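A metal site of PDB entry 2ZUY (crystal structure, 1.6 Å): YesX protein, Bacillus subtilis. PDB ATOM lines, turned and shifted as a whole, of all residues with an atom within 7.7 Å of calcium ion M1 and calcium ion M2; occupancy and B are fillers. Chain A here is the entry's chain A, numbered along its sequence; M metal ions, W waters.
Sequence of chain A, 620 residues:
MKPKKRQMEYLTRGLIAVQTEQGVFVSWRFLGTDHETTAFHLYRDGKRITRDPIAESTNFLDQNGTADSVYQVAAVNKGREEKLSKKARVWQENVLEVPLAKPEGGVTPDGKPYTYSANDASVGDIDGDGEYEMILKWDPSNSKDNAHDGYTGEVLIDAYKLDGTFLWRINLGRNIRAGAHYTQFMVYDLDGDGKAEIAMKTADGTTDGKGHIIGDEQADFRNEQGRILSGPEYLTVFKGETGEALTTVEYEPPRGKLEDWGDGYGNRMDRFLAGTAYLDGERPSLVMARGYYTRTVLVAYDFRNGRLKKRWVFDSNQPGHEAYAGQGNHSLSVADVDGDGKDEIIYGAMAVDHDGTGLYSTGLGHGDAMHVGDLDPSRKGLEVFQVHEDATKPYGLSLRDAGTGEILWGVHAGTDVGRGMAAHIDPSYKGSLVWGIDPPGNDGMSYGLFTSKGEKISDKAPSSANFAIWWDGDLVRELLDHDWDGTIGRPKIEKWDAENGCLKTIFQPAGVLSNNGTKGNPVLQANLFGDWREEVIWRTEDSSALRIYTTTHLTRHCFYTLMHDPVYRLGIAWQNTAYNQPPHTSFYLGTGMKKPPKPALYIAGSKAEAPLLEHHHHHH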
ATOM      1  N   LYS A   4       3.937  17.321  22.288  1.00  0.00           N
ATOM      2  CA  LYS A   4       4.274  16.623  21.048  1.00  0.00           C
ATOM      3  C   LYS A   4       2.987  16.293  20.292  1.00  0.00           C
ATOM      4  O   LYS A   4       1.970  15.981  20.908  1.00  0.00           O
ATOM      5  CB  LYS A   4       5.001  15.317  21.349  1.00  0.00           C
ATOM      6  CG  LYS A   4       6.398  15.454  21.929  1.00  0.00           C
ATOM      7  CD  LYS A   4       7.030  14.082  22.151  1.00  0.00           C
ATOM      8  CE  LYS A   4       6.731  13.530  23.537  1.00  0.00           C
ATOM      9  NZ  LYS A   4       7.647  14.086  24.565  1.00  0.00           N
ATOM     10  N   ARG A   6       0.947  13.747  18.112  1.00  0.00           N
ATOM     11  CA  ARG A   6       0.898  12.307  17.850  1.00  0.00           C
ATOM     12  C   ARG A   6       0.286  12.004  16.490  1.00  0.00           C
ATOM     13  O   ARG A   6      -0.699  12.617  16.084  1.00  0.00           O
ATOM     14  CB  ARG A   6       0.058  11.595  18.915  1.00  0.00           C
ATOM     15  CG  ARG A   6       0.741  11.514  20.255  1.00  0.00           C
ATOM     16  CD  ARG A   6      -0.043  10.635  21.225  1.00  0.00           C
ATOM     17  NE  ARG A   6       0.698  10.476  22.473  1.00  0.00           N
ATOM     18  CZ  ARG A   6       0.679   9.389  23.241  1.00  0.00           C
ATOM     19  NH1 ARG A   6      -0.052   8.330  22.911  1.00  0.00           N
ATOM     20  NH2 ARG A   6       1.426   9.366  24.345  1.00  0.00           N
ATOM     21  N   TYR A 278       2.769   4.773  22.074  1.00  0.00           N
ATOM     22  CA  TYR A 278       3.599   5.824  21.509  1.00  0.00           C
ATOM     23  C   TYR A 278       4.789   6.046  22.438  1.00  0.00           C
ATOM     24  O   TYR A 278       4.834   7.001  23.217  1.00  0.00           O
ATOM     25  CB  TYR A 278       2.796   7.126  21.316  1.00  0.00           C
ATOM     26  CG  TYR A 278       1.843   7.079  20.144  1.00  0.00           C
ATOM     27  CD1 TYR A 278       1.924   8.014  19.110  1.00  0.00           C
ATOM     28  CD2 TYR A 278       0.851   6.086  20.057  1.00  0.00           C
ATOM     29  CE1 TYR A 278       1.044   7.982  18.027  1.00  0.00           C
ATOM     30  CE2 TYR A 278      -0.034   6.041  18.978  1.00  0.00           C
ATOM     31  CZ  TYR A 278       0.075   6.989  17.964  1.00  0.00           C
ATOM     32  OH  TYR A 278      -0.787   6.944  16.909  1.00  0.00           O
ATOM     33  N   LEU A 279       5.762   5.149  22.342  1.00  0.00           N
ATOM     34  CA  LEU A 279       6.922   5.138  23.236  1.00  0.00           C
ATOM     35  C   LEU A 279       7.822   6.360  23.054  1.00  0.00           C
ATOM     36  O   LEU A 279       8.533   6.747  23.983  1.00  0.00           O
ATOM     37  CB  LEU A 279       7.689   3.814  23.096  1.00  0.00           C
ATOM     38  CG  LEU A 279       6.864   2.552  23.377  1.00  0.00           C
ATOM     39  CD1 LEU A 279       7.627   1.288  22.985  1.00  0.00           C
ATOM     40  CD2 LEU A 279       6.421   2.477  24.834  1.00  0.00           C
ATOM     41  N   ALA A 335      -0.766   4.538  28.508  1.00  0.00           N
ATOM     42  CA  ALA A 335      -1.026   5.963  28.731  1.00  0.00           C
ATOM     43  C   ALA A 335       0.256   6.672  29.107  1.00  0.00           C
ATOM     44  O   ALA A 335       1.181   6.051  29.649  1.00  0.00           O
ATOM     45  CB  ALA A 335      -2.054   6.152  29.832  1.00  0.00           C
ATOM     46  N   ASP A 336       0.292   7.979  28.843  1.00  0.00           N
ATOM     47  CA  ASP A 336       1.344   8.818  29.413  1.00  0.00           C
ATOM     48  C   ASP A 336       0.981   9.103  30.867  1.00  0.00           C
ATOM     49  O   ASP A 336       0.094   9.928  31.155  1.00  0.00           O
ATOM     50  CB  ASP A 336       1.516  10.110  28.616  1.00  0.00           C
ATOM     51  CG  ASP A 336       2.501  11.066  29.263  1.00  0.00           C
ATOM     52  OD1 ASP A 336       3.274  10.628  30.154  1.00  0.00           O
ATOM     53  OD2 ASP A 336       2.504  12.254  28.885  1.00  0.00           O
ATOM     54  N   VAL A 337       1.663   8.410  31.774  1.00  0.00           N
ATOM     55  CA  VAL A 337       1.326   8.476  33.201  1.00  0.00           C
ATOM     56  C   VAL A 337       2.260   9.376  34.013  1.00  0.00           C
ATOM     57  O   VAL A 337       1.978   9.691  35.175  1.00  0.00           O
ATOM     58  CB  VAL A 337       1.234   7.069  33.850  1.00  0.00           C
ATOM     59  CG1 VAL A 337       0.142   6.263  33.200  1.00  0.00           C
ATOM     60  CG2 VAL A 337       2.582   6.332  33.756  1.00  0.00           C
ATOM     61  N   ASP A 338       3.376   9.786  33.413  1.00  0.00           N
ATOM     62  CA  ASP A 338       4.382  10.570  34.134  1.00  0.00           C
ATOM     63  C   ASP A 338       4.605  11.972  33.555  1.00  0.00           C
ATOM     64  O   ASP A 338       5.485  12.700  34.020  1.00  0.00           O
ATOM     65  CB  ASP A 338       5.703   9.781  34.282  1.00  0.00           C
ATOM     66  CG  ASP A 338       6.336   9.411  32.949  1.00  0.00           C
ATOM     67  OD1 ASP A 338       5.876   9.896  31.890  1.00  0.00           O
ATOM     68  OD2 ASP A 338       7.304   8.627  32.961  1.00  0.00           O
ATOM     69  N   GLY A 339       3.816  12.342  32.554  1.00  0.00           N
ATOM     70  CA  GLY A 339       3.820  13.695  31.996  1.00  0.00           C
ATOM     71  C   GLY A 339       4.912  14.040  31.002  1.00  0.00           C
ATOM     72  O   GLY A 339       5.096  15.222  30.674  1.00  0.00           O
ATOM     73  N   ASP A 340       5.660  13.047  30.510  1.00  0.00           N
ATOM     74  CA  ASP A 340       6.725  13.317  29.544  1.00  0.00           C
ATOM     75  C   ASP A 340       6.286  13.223  28.079  1.00  0.00           C
ATOM     76  O   ASP A 340       7.116  13.319  27.168  1.00  0.00           O
ATOM     77  CB  ASP A 340       7.963  12.445  29.820  1.00  0.00           C
ATOM     78  CG  ASP A 340       7.695  10.961  29.655  1.00  0.00           C
ATOM     79  OD1 ASP A 340       6.642  10.589  29.079  1.00  0.00           O
ATOM     80  OD2 ASP A 340       8.536  10.147  30.109  1.00  0.00           O
ATOM     81  N   GLY A 341       4.991  13.007  27.862  1.00  0.00           N
ATOM     82  CA  GLY A 341       4.407  12.945  26.513  1.00  0.00           C
ATOM     83  C   GLY A 341       4.483  11.559  25.872  1.00  0.00           C
ATOM     84  O   GLY A 341       3.854  11.310  24.836  1.00  0.00           O
ATOM     85  N   LYS A 342       5.235  10.673  26.497  1.00  0.00           N
ATOM     86  CA  LYS A 342       5.477   9.332  25.966  1.00  0.00           C
ATOM     87  C   LYS A 342       4.629   8.316  26.717  1.00  0.00           C
ATOM     88  O   LYS A 342       4.357   8.483  27.898  1.00  0.00           O
ATOM     89  CB  LYS A 342       6.966   8.993  26.078  1.00  0.00           C
ATOM     90  CG  LYS A 342       7.879  10.019  25.397  1.00  0.00           C
ATOM     91  CD  LYS A 342       9.341   9.753  25.658  1.00  0.00           C
ATOM     92  CE  LYS A 342      10.202  10.848  25.048  1.00  0.00           C
ATOM     93  NZ  LYS A 342      11.653  10.598  25.276  1.00  0.00           N
ATOM     94  N   ASP A 343       4.205   7.259  26.024  1.00  0.00           N
ATOM     95  CA  ASP A 343       3.380   6.235  26.669  1.00  0.00           C
ATOM     96  C   ASP A 343       4.184   5.275  27.511  1.00  0.00           C
ATOM     97  O   ASP A 343       5.247   4.790  27.088  1.00  0.00           O
ATOM     98  CB  ASP A 343       2.586   5.416  25.651  1.00  0.00           C
ATOM     99  CG  ASP A 343       1.407   6.178  25.091  1.00  0.00           C
ATOM    100  OD1 ASP A 343       0.841   7.031  25.794  1.00  0.00           O
ATOM    101  OD2 ASP A 343       1.038   5.891  23.928  1.00  0.00           O
ATOM    102  N   GLU A 344       3.643   4.979  28.682  1.00  0.00           N
ATOM    103  CA  GLU A 344       4.103   3.860  29.509  1.00  0.00           C
ATOM    104  C   GLU A 344       3.115   2.702  29.370  1.00  0.00           C
ATOM    105  O   GLU A 344       1.978   2.889  28.911  1.00  0.00           O
ATOM    106  CB  GLU A 344       4.231   4.290  30.977  1.00  0.00           C
ATOM    107  CG  GLU A 344       5.432   5.210  31.261  1.00  0.00           C
ATOM    108  CD  GLU A 344       5.246   6.626  30.754  1.00  0.00           C
ATOM    109  OE1 GLU A 344       6.218   7.195  30.207  1.00  0.00           O
ATOM    110  OE2 GLU A 344       4.142   7.209  30.907  1.00  0.00           O
ATOM    111  N   VAL A 352       5.787  -0.547  33.073  1.00  0.00           N
ATOM    112  CA  VAL A 352       7.040  -0.456  32.346  1.00  0.00           C
ATOM    113  C   VAL A 352       7.155   0.940  31.713  1.00  0.00           C
ATOM    114  O   VAL A 352       6.190   1.443  31.114  1.00  0.00           O
ATOM    115  CB  VAL A 352       7.136  -1.563  31.271  1.00  0.00           C
ATOM    116  CG1 VAL A 352       8.385  -1.394  30.408  1.00  0.00           C
ATOM    117  CG2 VAL A 352       7.134  -2.942  31.933  1.00  0.00           C
ATOM    118  N   ASP A 353       8.313   1.573  31.869  1.00  0.00           N
ATOM    119  CA  ASP A 353       8.531   2.922  31.359  1.00  0.00           C
ATOM    120  C   ASP A 353       8.613   2.915  29.822  1.00  0.00           C
ATOM    121  O   ASP A 353       8.734   1.854  29.199  1.00  0.00           O
ATOM    122  CB  ASP A 353       9.802   3.520  31.985  1.00  0.00           C
ATOM    123  CG  ASP A 353       9.755   5.051  32.077  1.00  0.00           C
ATOM    124  OD1 ASP A 353       8.773   5.673  31.613  1.00  0.00           O
ATOM    125  OD2 ASP A 353      10.702   5.616  32.641  1.00  0.00           O
ATOM    126  N   HIS A 354       8.531   4.098  29.216  1.00  0.00           N
ATOM    127  CA  HIS A 354       8.530   4.234  27.746  1.00  0.00           C
ATOM    128  C   HIS A 354       9.794   3.669  27.086  1.00  0.00           C
ATOM    129  O   HIS A 354       9.787   3.382  25.889  1.00  0.00           O
ATOM    130  CB  HIS A 354       8.376   5.702  27.346  1.00  0.00           C
ATOM    131  CG  HIS A 354       9.560   6.541  27.676  1.00  0.00           C
ATOM    132  ND1 HIS A 354       9.677   7.244  28.857  1.00  0.00           N
ATOM    133  CD2 HIS A 354      10.707   6.774  26.994  1.00  0.00           C
ATOM    134  CE1 HIS A 354      10.843   7.873  28.880  1.00  0.00           C
ATOM    135  NE2 HIS A 354      11.482   7.604  27.763  1.00  0.00           N
ATOM    136  N   ASP A 355      10.864   3.537  27.867  1.00  0.00           N
ATOM    137  CA  ASP A 355      12.156   3.081  27.380  1.00  0.00           C
ATOM    138  C   ASP A 355      12.444   1.613  27.738  1.00  0.00           C
ATOM    139  O   ASP A 355      13.566   1.135  27.565  1.00  0.00           O
ATOM    140  CB  ASP A 355      13.278   4.002  27.893  1.00  0.00           C
ATOM    141  CG  ASP A 355      13.422   3.972  29.403  1.00  0.00           C
ATOM    142  OD1 ASP A 355      12.609   3.315  30.082  1.00  0.00           O
ATOM    143  OD2 ASP A 355      14.376   4.615  29.924  1.00  0.00           O
ATOM    144  N   THR A 357      12.468   0.242  30.696  1.00  0.00           N
ATOM    145  CA  THR A 357      12.936   0.071  32.076  1.00  0.00           C
ATOM    146  C   THR A 357      11.717  -0.093  32.981  1.00  0.00           C
ATOM    147  O   THR A 357      10.607   0.273  32.603  1.00  0.00           O
ATOM    148  CB  THR A 357      13.786   1.255  32.561  1.00  0.00           C
ATOM    149  OG1 THR A 357      13.008   2.458  32.556  1.00  0.00           O
ATOM    150  CG2 THR A 357      15.036   1.434  31.684  1.00  0.00           C
ATOM    151  N   LEU A 359       9.102   0.865  35.606  1.00  0.00           N
ATOM    152  CA  LEU A 359       8.590   2.104  36.179  1.00  0.00           C
ATOM    153  C   LEU A 359       8.323   1.888  37.663  1.00  0.00           C
ATOM    154  O   LEU A 359       8.923   2.550  38.518  1.00  0.00           O
ATOM    155  CB  LEU A 359       7.330   2.594  35.448  1.00  0.00           C
ATOM    156  CG  LEU A 359       6.867   4.034  35.726  1.00  0.00           C
ATOM    157  CD1 LEU A 359       7.847   5.085  35.178  1.00  0.00           C
ATOM    158  CD2 LEU A 359       5.476   4.280  35.156  1.00  0.00           C
HETATM  159 CA    CA M   1       8.306   7.948  30.891  1.00  0.00          CA
HETATM  160 CA    CA M   2       5.067   9.233  29.877  1.00  0.00          CA
HETATM  161  O   HOH W   1      10.338   8.322  32.024  1.00  0.00           O
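Val 337 touches calcium ion M2.
The nearest printed residue that does not touch calcium ion M2 is Gly 341 (4.3 Å).
NZ of Lys 4 is in hydrogen-bond range of O of Asp 340 (2.8 Å).
The side-chain carboxylate of Asp 336 lies within hydrogen-bond range of the backbone NH of Gly 341 (2.8 Å).
The side-chain carboxylate of Asp 336 lies close to the backbone NH of Gly 339 (3.0 Å).
The backbone NH (N) of Asp 336 is in hydrogen-bond range of the side-chain carboxylate (OD1) of Asp 343 (3.2 Å).
N of Val 337 sits close to OE2 of Glu 344.
The backbone NH (N) of Glu 344 lies within hydrogen-bond range of the backbone carbonyl oxygen (O) of Ala 335 (2.9 Å).
Calcium ion M2 is bound by OD1 of Asp 340 (2.2 Å), O of Lys 342 (2.2 Å), OD1 of Asp 338 (2.3 Å), OD1 of Asp 336 (2.3 Å), OE1 of Glu 344 (2.4 Å) and OE2 of Glu 344 (2.5 Å).
OE1 of Glu 344 binds calcium ion M1 (2.3 Å).
The side-chain carboxylate (OD2) of Asp 340 is bound to calcium ion M1 (2.3 Å).
Calcium ion M1 is bound by water W1 (2.4 Å).
Calcium ion M1 is bound by the side-chain carboxylate (OD2) of Asp 338.
The side-chain carboxylate (OD1) of Asp 353 is bound to calcium ion M1 (2.4 Å).
Calcium ion M1 is bound by ND1 of His 354.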
